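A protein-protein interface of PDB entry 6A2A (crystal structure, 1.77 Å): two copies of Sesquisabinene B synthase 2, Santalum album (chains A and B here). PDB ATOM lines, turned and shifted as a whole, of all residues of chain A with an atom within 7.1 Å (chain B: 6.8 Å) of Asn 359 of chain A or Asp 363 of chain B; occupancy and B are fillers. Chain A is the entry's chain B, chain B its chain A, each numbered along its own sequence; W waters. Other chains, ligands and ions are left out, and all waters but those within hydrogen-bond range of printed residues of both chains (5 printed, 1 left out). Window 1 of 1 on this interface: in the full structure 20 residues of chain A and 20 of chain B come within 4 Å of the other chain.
The side-chain hydroxyl of Tyr 366 of chain B lies within hydrogen-bond range of the side-chain hydroxyl of Thr 356 of chain A (2.9 Å).
The backbone carbonyl oxygen (O) of Ile 377 of chain B sits at hydrogen-bond distance from the side-chain hydroxyl (OG1) of Thr 380 of chain B (3.3 Å). The side-chain amide nitrogen (ND2) of Asn 362 of chain B sits close to the backbone carbonyl oxygen (O) of Phe 358 of chain B (3.2 Å). NE1 of Trp 338 of chain A lies within hydrogen-bond range of OD1 of Asn 362 of chain A, 2.8 Å away. The backbone carbonyl oxygen (O) of Phe 358 of chain A lies close to the side-chain amide nitrogen (ND2) of Asn 362 of chain A (3.2 Å). O of Leu 355 of chain A lies close to ND2 of Asn 359 of chain A (3.5 Å). OG1 of Thr 360 of chain A lies within hydrogen-bond range of O of Thr 356 of chain A (3.2 Å).
Ile 340 of chain A touches Ile 377 of chain B (CD1 to CD1, 3.7 Å). CB of Leu 355 of chain A touches CD2 of Tyr 366 of chain B (3.6 Å). CZ of Phe 358 of chain A touches CZ of Phe 358 of chain B, at 3.96 Å. Phe 358 of chain A touches Asn 362 of chain B. Asn 359 of chain A touches Asn 362 of chain B. Asn 359 of chain A touches Asp 363 of chain B. Tyr 366 of chain B touches Asn 359 of chain A. Asn 362 of chain A touches Phe 358 of chain B. Asn 359 of chain B touches Asn 362 of chain A. Asp 363 of chain A touches Asn 359 of chain B.
Of chain B, only Asn 362, Asp 363 and Tyr 366 come within 4 Å of Asn 359 of chain A. Of chain A, only Asn 359 (3.9 Å) comes within 4 Å of Asp 363 of chain B. Of the printed residues of chain A, Ile 377 of chain B touches Ile 340 (3.7 Å). Printed residues of chain B within 4 Å of Phe 358 of chain A: Phe 358 (3.96 Å) and Asn 362 (3.6 Å). The nearest residue of chain B that does not touch Asn 359 of chain A is Ile 377 of chain B (5.0 Å). The nearest printed residue of chain A that does not touch Ile 377 of chain B is Leu 355 of chain A (4.4 Å).
Hydrophobic or aromatic side chains of chain B within 4 Å of the printed part of chain A: Phe 358, Tyr 366 and Ile 377. Of the 17 printed residues of chain A, 7 touch a printed residue of chain B. Hydrophobic or aromatic side chains of chain A within 4 Å of the printed part of chain B: Ile 340, Leu 355 and Phe 358. Along chain A the printed residues that touch a printed residue of chain B span positions 340 to 363. Among the printed residues, 11 pairs touch across the chains. Among the printed residues, no Asp or Glu carboxylate lies within 4 Å of a Lys or Arg side-chain nitrogen of the other chain.
Phe 358 of chain B touches its own counterpart, Phe 358 of chain A. Phe 358 of chain A touches Asn 362 of chain B, and with the chains exchanged Asn 362 of chain A touches Phe 358 of chain B. Asn 359 of chain A touches Asn 362 of chain B, and with the chains exchanged Asn 362 of chain A touches Asn 359 of chain B. Asn 359 of chain A touches Asp 363 of chain B, and with the chains exchanged Asp 363 of chain A touches Asn 359 of chain B. 9 positions are printed for both chains.
Water W4 bridges OD2 of Asp 363 of chain B and OD1 of Asp 363 of chain A. Water W1 bridges OD1 of Asp 363 of chain B (2.6 Å) and OD2 of Asp 363 of chain A (2.7 Å). Water W3 lies within hydrogen-bond range of OD1 of Asp 363 of chain B (2.9 Å) and ND2 of Asn 359 of chain A (3.1 Å). Water W2 lies within hydrogen-bond range of the side-chain amide nitrogen of Asn 362 of chain B (3.0 Å), the side-chain amide nitrogen of Asn 362 of chain A (3.0 Å), the side-chain amide oxygen of Asn 359 of chain B (3.2 Å) and the side-chain amide oxygen of Asn 359 of chain A (3.3 Å). Water W5 bridges OD1 of Asp 363 of chain A (3.0 Å) and ND2 of Asn 359 of chain B (3.2 Å).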
ATOM      1  N   TRP A 266      32.095  12.846   0.950  1.00  0.00           N
ATOM      2  CA  TRP A 266      31.056  11.923   0.670  1.00  0.00           C
ATOM      3  C   TRP A 266      29.824  12.163   1.561  1.00  0.00           C
ATOM      4  O   TRP A 266      28.676  12.241   1.099  1.00  0.00           O
ATOM      5  CB  TRP A 266      31.597  10.488   0.812  1.00  0.00           C
ATOM      6  CG  TRP A 266      30.514   9.476   0.801  1.00  0.00           C
ATOM      7  CD1 TRP A 266      29.798   9.045  -0.279  1.00  0.00           C
ATOM      8  CD2 TRP A 266      29.999   8.753   1.937  1.00  0.00           C
ATOM      9  NE1 TRP A 266      28.860   8.148   0.104  1.00  0.00           N
ATOM     10  CE2 TRP A 266      28.970   7.931   1.466  1.00  0.00           C
ATOM     11  CE3 TRP A 266      30.309   8.743   3.306  1.00  0.00           C
ATOM     12  CZ2 TRP A 266      28.242   7.085   2.301  1.00  0.00           C
ATOM     13  CZ3 TRP A 266      29.605   7.886   4.122  1.00  0.00           C
ATOM     14  CH2 TRP A 266      28.575   7.089   3.649  1.00  0.00           C
ATOM     15  N   LEU A 311      26.502   4.309   8.055  1.00  0.00           N
ATOM     16  CA  LEU A 311      25.145   4.086   7.675  1.00  0.00           C
ATOM     17  C   LEU A 311      24.402   3.205   8.699  1.00  0.00           C
ATOM     18  O   LEU A 311      23.197   3.293   8.838  1.00  0.00           O
ATOM     19  CB  LEU A 311      25.116   3.425   6.295  1.00  0.00           C
ATOM     20  CG  LEU A 311      25.386   4.400   5.147  1.00  0.00           C
ATOM     21  CD1 LEU A 311      25.616   3.616   3.851  1.00  0.00           C
ATOM     22  CD2 LEU A 311      24.237   5.373   5.005  1.00  0.00           C
ATOM     23  N   TRP A 338      15.611  -5.161  -3.392  1.00  0.00           N
ATOM     24  CA  TRP A 338      16.591  -4.276  -4.079  1.00  0.00           C
ATOM     25  C   TRP A 338      15.919  -3.554  -5.250  1.00  0.00           C
ATOM     26  O   TRP A 338      16.402  -3.550  -6.379  1.00  0.00           O
ATOM     27  CB  TRP A 338      17.840  -5.043  -4.513  1.00  0.00           C
ATOM     28  CG  TRP A 338      19.124  -4.270  -4.414  1.00  0.00           C
ATOM     29  CD1 TRP A 338      20.003  -3.994  -5.426  1.00  0.00           C
ATOM     30  CD2 TRP A 338      19.712  -3.739  -3.220  1.00  0.00           C
ATOM     31  NE1 TRP A 338      21.092  -3.319  -4.941  1.00  0.00           N
ATOM     32  CE2 TRP A 338      20.926  -3.126  -3.592  1.00  0.00           C
ATOM     33  CE3 TRP A 338      19.316  -3.691  -1.881  1.00  0.00           C
ATOM     34  CZ2 TRP A 338      21.746  -2.491  -2.661  1.00  0.00           C
ATOM     35  CZ3 TRP A 338      20.128  -3.067  -0.963  1.00  0.00           C
ATOM     36  CH2 TRP A 338      21.328  -2.467  -1.347  1.00  0.00           C
ATOM     37  N   ILE A 340      13.970   0.184  -5.810  1.00  0.00           N
ATOM     38  CA  ILE A 340      13.721   1.503  -5.250  1.00  0.00           C
ATOM     39  C   ILE A 340      12.543   2.183  -5.957  1.00  0.00           C
ATOM     40  O   ILE A 340      12.325   3.380  -5.785  1.00  0.00           O
ATOM     41  CB  ILE A 340      14.998   2.362  -5.320  1.00  0.00           C
ATOM     42  CG1 ILE A 340      15.552   2.515  -6.741  1.00  0.00           C
ATOM     43  CG2 ILE A 340      16.045   1.811  -4.389  1.00  0.00           C
ATOM     44  CD1 ILE A 340      16.612   3.630  -6.854  1.00  0.00           C
ATOM     45  N   PRO A 353      18.370   8.292   3.857  1.00  0.00           N
ATOM     46  CA  PRO A 353      19.174   7.175   4.312  1.00  0.00           C
ATOM     47  C   PRO A 353      19.010   5.900   3.470  1.00  0.00           C
ATOM     48  O   PRO A 353      20.002   5.171   3.261  1.00  0.00           O
ATOM     49  CB  PRO A 353      18.712   6.894   5.762  1.00  0.00           C
ATOM     50  CG  PRO A 353      17.763   8.004   6.125  1.00  0.00           C
ATOM     51  CD  PRO A 353      17.597   8.929   4.944  1.00  0.00           C
ATOM     52  N   LEU A 354      17.807   5.618   3.020  1.00  0.00           N
ATOM     53  CA  LEU A 354      17.559   4.415   2.269  1.00  0.00           C
ATOM     54  C   LEU A 354      18.336   4.449   0.941  1.00  0.00           C
ATOM     55  O   LEU A 354      18.995   3.505   0.590  1.00  0.00           O
ATOM     56  CB  LEU A 354      16.074   4.327   1.947  1.00  0.00           C
ATOM     57  CG  LEU A 354      15.684   3.301   0.886  1.00  0.00           C
ATOM     58  CD1 LEU A 354      15.734   1.888   1.445  1.00  0.00           C
ATOM     59  CD2 LEU A 354      14.317   3.596   0.324  1.00  0.00           C
ATOM     60  N   LEU A 355      18.162   5.531   0.192  1.00  0.00           N
ATOM     61  CA  LEU A 355      18.843   5.619  -1.120  1.00  0.00           C
ATOM     62  C   LEU A 355      20.350   5.684  -0.909  1.00  0.00           C
ATOM     63  O   LEU A 355      21.103   5.157  -1.745  1.00  0.00           O
ATOM     64  CB  LEU A 355      18.267   6.783  -1.941  1.00  0.00           C
ATOM     65  CG  LEU A 355      16.812   6.628  -2.373  1.00  0.00           C
ATOM     66  CD1 LEU A 355      16.305   7.890  -3.048  1.00  0.00           C
ATOM     67  CD2 LEU A 355      16.620   5.452  -3.312  1.00  0.00           C
ATOM     68  N   THR A 356      20.834   6.231   0.221  1.00  0.00           N
ATOM     69  CA  THR A 356      22.251   6.252   0.456  1.00  0.00           C
ATOM     70  C   THR A 356      22.732   4.825   0.717  1.00  0.00           C
ATOM     71  O   THR A 356      23.796   4.478   0.251  1.00  0.00           O
ATOM     72  CB  THR A 356      22.686   7.275   1.520  1.00  0.00           C
ATOM     73  OG1 THR A 356      22.422   8.608   1.048  1.00  0.00           O
ATOM     74  CG2 THR A 356      24.156   7.167   1.849  1.00  0.00           C
ATOM     75  N   MET A 357      21.980   4.051   1.516  1.00  0.00           N
ATOM     76  CA  MET A 357      22.312   2.654   1.767  1.00  0.00           C
ATOM     77  C   MET A 357      22.404   1.830   0.472  1.00  0.00           C
ATOM     78  O   MET A 357      23.356   1.063   0.293  1.00  0.00           O
ATOM     79  CB  MET A 357      21.248   2.002   2.649  1.00  0.00           C
ATOM     80  CG  MET A 357      21.457   0.505   2.813  1.00  0.00           C
ATOM     81  SD  MET A 357      19.922  -0.284   3.363  1.00  0.00           S
ATOM     82  CE  MET A 357      18.870  -0.012   1.942  1.00  0.00           C
ATOM     83  N   PHE A 358      21.422   2.000  -0.345  1.00  0.00           N
ATOM     84  CA  PHE A 358      21.308   1.363  -1.707  1.00  0.00           C
ATOM     85  C   PHE A 358      22.497   1.758  -2.584  1.00  0.00           C
ATOM     86  O   PHE A 358      23.258   0.886  -3.061  1.00  0.00           O
ATOM     87  CB  PHE A 358      19.985   1.822  -2.307  1.00  0.00           C
ATOM     88  CG  PHE A 358      19.640   1.218  -3.637  1.00  0.00           C
ATOM     89  CD1 PHE A 358      19.270  -0.112  -3.739  1.00  0.00           C
ATOM     90  CD2 PHE A 358      19.705   1.988  -4.786  1.00  0.00           C
ATOM     91  CE1 PHE A 358      18.944  -0.659  -4.967  1.00  0.00           C
ATOM     92  CE2 PHE A 358      19.385   1.435  -6.017  1.00  0.00           C
ATOM     93  CZ  PHE A 358      18.999   0.122  -6.102  1.00  0.00           C
ATOM     94  N   ASN A 359      22.699   3.083  -2.746  1.00  0.00           N
ATOM     95  CA  ASN A 359      23.795   3.561  -3.595  1.00  0.00           C
ATOM     96  C   ASN A 359      25.159   3.106  -3.076  1.00  0.00           C
ATOM     97  O   ASN A 359      26.012   2.618  -3.883  1.00  0.00           O
ATOM     98  CB  ASN A 359      23.719   5.085  -3.779  1.00  0.00           C
ATOM     99  CG  ASN A 359      22.508   5.541  -4.552  1.00  0.00           C
ATOM    100  OD1 ASN A 359      21.794   4.764  -5.148  1.00  0.00           O
ATOM    101  ND2 ASN A 359      22.249   6.836  -4.550  1.00  0.00           N
ATOM    102  N   THR A 360      25.425   3.168  -1.750  1.00  0.00           N
ATOM    103  CA  THR A 360      26.687   2.815  -1.231  1.00  0.00           C
ATOM    104  C   THR A 360      26.861   1.291  -1.297  1.00  0.00           C
ATOM    105  O   THR A 360      27.950   0.822  -1.579  1.00  0.00           O
ATOM    106  CB  THR A 360      26.832   3.337   0.223  1.00  0.00           C
ATOM    107  OG1 THR A 360      26.986   4.763   0.162  1.00  0.00           O
ATOM    108  CG2 THR A 360      28.004   2.730   0.945  1.00  0.00           C
ATOM    109  N   SER A 361      25.791   0.539  -1.121  1.00  0.00           N
ATOM    110  CA  SER A 361      25.929  -0.925  -1.190  1.00  0.00           C
ATOM    111  C   SER A 361      26.247  -1.344  -2.623  1.00  0.00           C
ATOM    112  O   SER A 361      27.035  -2.219  -2.833  1.00  0.00           O
ATOM    113  CB  SER A 361      24.720  -1.650  -0.687  1.00  0.00           C
ATOM    114  OG  SER A 361      24.513  -1.431   0.709  1.00  0.00           O
ATOM    115  N   ASN A 362      25.621  -0.648  -3.576  1.00  0.00           N
ATOM    116  CA  ASN A 362      25.903  -0.824  -5.001  1.00  0.00           C
ATOM    117  C   ASN A 362      27.349  -0.470  -5.275  1.00  0.00           C
ATOM    118  O   ASN A 362      28.028  -1.214  -5.967  1.00  0.00           O
ATOM    119  CB  ASN A 362      24.897  -0.040  -5.848  1.00  0.00           C
ATOM    120  CG  ASN A 362      23.525  -0.666  -5.845  1.00  0.00           C
ATOM    121  OD1 ASN A 362      23.405  -1.867  -5.633  1.00  0.00           O
ATOM    122  ND2 ASN A 362      22.483   0.114  -6.083  1.00  0.00           N
ATOM    123  N   ASP A 363      27.858   0.674  -4.763  1.00  0.00           N
ATOM    124  CA  ASP A 363      29.241   1.009  -4.920  1.00  0.00           C
ATOM    125  C   ASP A 363      30.225  -0.017  -4.392  1.00  0.00           C
ATOM    126  O   ASP A 363      31.243  -0.290  -4.983  1.00  0.00           O
ATOM    127  CB  ASP A 363      29.547   2.365  -4.235  1.00  0.00           C
ATOM    128  CG  ASP A 363      28.951   3.577  -4.951  1.00  0.00           C
ATOM    129  OD1 ASP A 363      28.579   3.496  -6.155  1.00  0.00           O
ATOM    130  OD2 ASP A 363      28.889   4.647  -4.271  1.00  0.00           O
ATOM    131  N   ILE A 364      29.956  -0.545  -3.201  1.00  0.00           N
ATOM    132  CA  ILE A 364      30.898  -1.447  -2.562  1.00  0.00           C
ATOM    133  C   ILE A 364      30.864  -2.786  -3.313  1.00  0.00           C
ATOM    134  O   ILE A 364      31.883  -3.345  -3.598  1.00  0.00           O
ATOM    135  CB  ILE A 364      30.526  -1.602  -1.062  1.00  0.00           C
ATOM    136  CG1 ILE A 364      30.848  -0.350  -0.247  1.00  0.00           C
ATOM    137  CG2 ILE A 364      31.201  -2.839  -0.475  1.00  0.00           C
ATOM    138  CD1 ILE A 364      30.185  -0.371   1.124  1.00  0.00           C
ATOM    139  N   GLY A 365      29.684  -3.238  -3.639  1.00  0.00           N
ATOM    140  CA  GLY A 365      29.526  -4.455  -4.474  1.00  0.00           C
ATOM    141  C   GLY A 365      30.275  -4.330  -5.797  1.00  0.00           C
ATOM    142  O   GLY A 365      30.878  -5.275  -6.309  1.00  0.00           O
ATOM    143  N   TRP B 266      37.403   9.380 -10.065  1.00  0.00           N
ATOM    144  CA  TRP B 266      36.156   8.668 -10.218  1.00  0.00           C
ATOM    145  C   TRP B 266      36.293   7.606 -11.333  1.00  0.00           C
ATOM    146  O   TRP B 266      35.841   6.473 -11.164  1.00  0.00           O
ATOM    147  CB  TRP B 266      35.007   9.638 -10.539  1.00  0.00           C
ATOM    148  CG  TRP B 266      33.768   8.971 -11.045  1.00  0.00           C
ATOM    149  CD1 TRP B 266      32.833   8.292 -10.313  1.00  0.00           C
ATOM    150  CD2 TRP B 266      33.316   8.929 -12.420  1.00  0.00           C
ATOM    151  NE1 TRP B 266      31.855   7.795 -11.130  1.00  0.00           N
ATOM    152  CE2 TRP B 266      32.114   8.188 -12.433  1.00  0.00           C
ATOM    153  CE3 TRP B 266      33.817   9.439 -13.623  1.00  0.00           C
ATOM    154  CZ2 TRP B 266      31.401   7.930 -13.604  1.00  0.00           C
ATOM    155  CZ3 TRP B 266      33.092   9.191 -14.779  1.00  0.00           C
ATOM    156  CH2 TRP B 266      31.893   8.481 -14.761  1.00  0.00           C
ATOM    157  N   MET B 304      28.846  16.326 -13.268  1.00  0.00           N
ATOM    158  CA  MET B 304      27.882  15.302 -13.455  1.00  0.00           C
ATOM    159  C   MET B 304      27.642  15.156 -14.965  1.00  0.00           C
ATOM    160  O   MET B 304      27.488  14.002 -15.475  1.00  0.00           O
ATOM    161  CB  MET B 304      26.601  15.562 -12.665  1.00  0.00           C
ATOM    162  CG  MET B 304      26.753  15.241 -11.168  1.00  0.00           C
ATOM    163  SD  MET B 304      25.239  15.523 -10.262  1.00  0.00           S
ATOM    164  CE  MET B 304      25.391  17.278  -9.901  1.00  0.00           C
ATOM    165  N   LYS B 307      30.403  13.116 -16.379  1.00  0.00           N
ATOM    166  CA  LYS B 307      30.277  11.673 -16.079  1.00  0.00           C
ATOM    167  C   LYS B 307      29.286  11.022 -17.047  1.00  0.00           C
ATOM    168  O   LYS B 307      29.587   9.968 -17.637  1.00  0.00           O
ATOM    169  CB  LYS B 307      29.791  11.432 -14.656  1.00  0.00           C
ATOM    170  CG  LYS B 307      30.754  11.815 -13.547  1.00  0.00           C
ATOM    171  CD  LYS B 307      30.187  11.439 -12.197  1.00  0.00           C
ATOM    172  CE  LYS B 307      31.163  11.657 -11.058  1.00  0.00           C
ATOM    173  NZ  LYS B 307      30.518  11.231  -9.776  1.00  0.00           N
ATOM    174  N   PHE B 358      24.246   2.505 -14.086  1.00  0.00           N
ATOM    175  CA  PHE B 358      23.226   2.372 -13.073  1.00  0.00           C
ATOM    176  C   PHE B 358      23.610   3.190 -11.808  1.00  0.00           C
ATOM    177  O   PHE B 358      22.822   3.984 -11.343  1.00  0.00           O
ATOM    178  CB  PHE B 358      23.067   0.873 -12.776  1.00  0.00           C
ATOM    179  CG  PHE B 358      22.030   0.523 -11.747  1.00  0.00           C
ATOM    180  CD1 PHE B 358      20.702   0.564 -12.080  1.00  0.00           C
ATOM    181  CD2 PHE B 358      22.391   0.202 -10.447  1.00  0.00           C
ATOM    182  CE1 PHE B 358      19.728   0.231 -11.158  1.00  0.00           C
ATOM    183  CE2 PHE B 358      21.411  -0.137  -9.533  1.00  0.00           C
ATOM    184  CZ  PHE B 358      20.100  -0.132  -9.901  1.00  0.00           C
ATOM    185  N   ASN B 359      24.819   2.998 -11.310  1.00  0.00           N
ATOM    186  CA  ASN B 359      25.309   3.600 -10.072  1.00  0.00           C
ATOM    187  C   ASN B 359      25.417   5.128 -10.229  1.00  0.00           C
ATOM    188  O   ASN B 359      24.995   5.886  -9.341  1.00  0.00           O
ATOM    189  CB  ASN B 359      26.637   3.022  -9.587  1.00  0.00           C
ATOM    190  CG  ASN B 359      26.533   1.585  -9.103  1.00  0.00           C
ATOM    191  OD1 ASN B 359      25.443   1.074  -8.952  1.00  0.00           O
ATOM    192  ND2 ASN B 359      27.664   0.930  -8.952  1.00  0.00           N
ATOM    193  N   THR B 360      25.929   5.597 -11.369  1.00  0.00           N
ATOM    194  CA  THR B 360      26.068   7.000 -11.601  1.00  0.00           C
ATOM    195  C   THR B 360      24.694   7.680 -11.763  1.00  0.00           C
ATOM    196  O   THR B 360      24.468   8.827 -11.239  1.00  0.00           O
ATOM    197  CB  THR B 360      26.990   7.226 -12.800  1.00  0.00           C
ATOM    198  OG1 THR B 360      28.313   6.796 -12.460  1.00  0.00           O
ATOM    199  CG2 THR B 360      27.017   8.679 -13.214  1.00  0.00           C
ATOM    200  N   SER B 361      23.774   7.043 -12.503  1.00  0.00           N
ATOM    201  CA  SER B 361      22.419   7.570 -12.676  1.00  0.00           C
ATOM    202  C   SER B 361      21.716   7.706 -11.309  1.00  0.00           C
ATOM    203  O   SER B 361      21.033   8.666 -11.066  1.00  0.00           O
ATOM    204  CB  SER B 361      21.625   6.731 -13.612  1.00  0.00           C
ATOM    205  OG  SER B 361      22.233   6.824 -14.892  1.00  0.00           O
ATOM    206  N   ASN B 362      21.886   6.713 -10.458  1.00  0.00           N
ATOM    207  CA  ASN B 362      21.375   6.770  -9.076  1.00  0.00           C
ATOM    208  C   ASN B 362      22.040   7.897  -8.269  1.00  0.00           C
ATOM    209  O   ASN B 362      21.324   8.577  -7.518  1.00  0.00           O
ATOM    210  CB  ASN B 362      21.521   5.414  -8.397  1.00  0.00           C
ATOM    211  CG  ASN B 362      20.636   4.348  -9.012  1.00  0.00           C
ATOM    212  OD1 ASN B 362      19.609   4.657  -9.599  1.00  0.00           O
ATOM    213  ND2 ASN B 362      21.017   3.084  -8.825  1.00  0.00           N
ATOM    214  N   ASP B 363      23.366   8.060  -8.342  1.00  0.00           N
ATOM    215  CA  ASP B 363      24.054   9.159  -7.742  1.00  0.00           C
ATOM    216  C   ASP B 363      23.538  10.527  -8.188  1.00  0.00           C
ATOM    217  O   ASP B 363      23.273  11.438  -7.375  1.00  0.00           O
ATOM    218  CB  ASP B 363      25.565   9.088  -8.003  1.00  0.00           C
ATOM    219  CG  ASP B 363      26.285   7.981  -7.248  1.00  0.00           C
ATOM    220  OD1 ASP B 363      25.730   7.443  -6.258  1.00  0.00           O
ATOM    221  OD2 ASP B 363      27.477   7.682  -7.619  1.00  0.00           O
ATOM    222  N   ILE B 364      23.320  10.687  -9.494  1.00  0.00           N
ATOM    223  CA  ILE B 364      22.860  11.977 -10.046  1.00  0.00           C
ATOM    224  C   ILE B 364      21.430  12.253  -9.592  1.00  0.00           C
ATOM    225  O   ILE B 364      21.106  13.362  -9.149  1.00  0.00           O
ATOM    226  CB  ILE B 364      23.002  11.994 -11.578  1.00  0.00           C
ATOM    227  CG1 ILE B 364      24.489  12.004 -11.939  1.00  0.00           C
ATOM    228  CG2 ILE B 364      22.282  13.183 -12.194  1.00  0.00           C
ATOM    229  CD1 ILE B 364      24.839  11.855 -13.404  1.00  0.00           C
ATOM    230  N   GLY B 365      20.564  11.242  -9.678  1.00  0.00           N
ATOM    231  CA  GLY B 365      19.179  11.416  -9.224  1.00  0.00           C
ATOM    232  C   GLY B 365      19.124  11.728  -7.740  1.00  0.00           C
ATOM    233  O   GLY B 365      18.257  12.538  -7.285  1.00  0.00           O
ATOM    234  N   TYR B 366      20.003  11.109  -6.975  1.00  0.00           N
ATOM    235  CA  TYR B 366      20.073  11.328  -5.546  1.00  0.00           C
ATOM    236  C   TYR B 366      20.534  12.771  -5.247  1.00  0.00           C
ATOM    237  O   TYR B 366      20.009  13.439  -4.325  1.00  0.00           O
ATOM    238  CB  TYR B 366      20.981  10.302  -4.882  1.00  0.00           C
ATOM    239  CG  TYR B 366      21.000  10.500  -3.387  1.00  0.00           C
ATOM    240  CD1 TYR B 366      21.853  11.411  -2.796  1.00  0.00           C
ATOM    241  CD2 TYR B 366      20.104   9.812  -2.593  1.00  0.00           C
ATOM    242  CE1 TYR B 366      21.859  11.594  -1.421  1.00  0.00           C
ATOM    243  CE2 TYR B 366      20.120   9.963  -1.220  1.00  0.00           C
ATOM    244  CZ  TYR B 366      20.982  10.870  -0.638  1.00  0.00           C
ATOM    245  OH  TYR B 366      20.931  11.099   0.716  1.00  0.00           O
ATOM    246  N   TRP B 367      21.510  13.278  -5.992  1.00  0.00           N
ATOM    247  CA  TRP B 367      21.973  14.663  -5.797  1.00  0.00           C
ATOM    248  C   TRP B 367      20.763  15.592  -5.949  1.00  0.00           C
ATOM    249  O   TRP B 367      20.621  16.572  -5.195  1.00  0.00           O
ATOM    250  CB  TRP B 367      23.046  15.034  -6.835  1.00  0.00           C
ATOM    251  CG  TRP B 367      23.665  16.392  -6.676  1.00  0.00           C
ATOM    252  CD1 TRP B 367      24.860  16.660  -6.094  1.00  0.00           C
ATOM    253  CD2 TRP B 367      23.190  17.656  -7.197  1.00  0.00           C
ATOM    254  NE1 TRP B 367      25.182  17.983  -6.223  1.00  0.00           N
ATOM    255  CE2 TRP B 367      24.160  18.627  -6.859  1.00  0.00           C
ATOM    256  CE3 TRP B 367      22.048  18.060  -7.890  1.00  0.00           C
ATOM    257  CZ2 TRP B 367      24.027  19.970  -7.214  1.00  0.00           C
ATOM    258  CZ3 TRP B 367      21.899  19.395  -8.225  1.00  0.00           C
ATOM    259  CH2 TRP B 367      22.882  20.327  -7.888  1.00  0.00           C
ATOM    260  N   ALA B 368      19.914  15.348  -6.933  1.00  0.00           N
ATOM    261  CA  ALA B 368      18.729  16.166  -7.118  1.00  0.00           C
ATOM    262  C   ALA B 368      17.821  16.064  -5.884  1.00  0.00           C
ATOM    263  O   ALA B 368      17.207  17.066  -5.458  1.00  0.00           O
ATOM    264  CB  ALA B 368      17.962  15.801  -8.380  1.00  0.00           C
ATOM    265  N   ILE B 377      16.024  10.056  -9.817  1.00  0.00           N
ATOM    266  CA  ILE B 377      16.380   8.721 -10.383  1.00  0.00           C
ATOM    267  C   ILE B 377      15.398   8.284 -11.476  1.00  0.00           C
ATOM    268  O   ILE B 377      15.845   7.710 -12.469  1.00  0.00           O
ATOM    269  CB  ILE B 377      16.532   7.661  -9.291  1.00  0.00           C
ATOM    270  CG1 ILE B 377      17.676   8.069  -8.356  1.00  0.00           C
ATOM    271  CG2 ILE B 377      16.713   6.273  -9.927  1.00  0.00           C
ATOM    272  CD1 ILE B 377      17.916   7.090  -7.239  1.00  0.00           C
ATOM    273  N   THR B 380      16.677  10.103 -14.715  1.00  0.00           N
ATOM    274  CA  THR B 380      17.920   9.607 -15.292  1.00  0.00           C
ATOM    275  C   THR B 380      17.694   8.195 -15.854  1.00  0.00           C
ATOM    276  O   THR B 380      18.222   7.844 -16.884  1.00  0.00           O
ATOM    277  CB  THR B 380      19.078   9.689 -14.280  1.00  0.00           C
ATOM    278  OG1 THR B 380      18.807   8.908 -13.108  1.00  0.00           O
ATOM    279  CG2 THR B 380      19.285  11.123 -13.842  1.00  0.00           C
HETATM  280  O   HOH W   1      26.955   6.549  -4.088  1.00  0.00           O
HETATM  281  O   HOH W   2      23.414   2.736  -7.134  1.00  0.00           O
HETATM  282  O   HOH W   3      24.541   8.945  -4.085  1.00  0.00           O
HETATM  283  O   HOH W   4      28.700   5.534  -7.936  1.00  0.00           O
HETATM  284  O   HOH W   5      30.420   2.412  -8.244  1.00  0.00           O
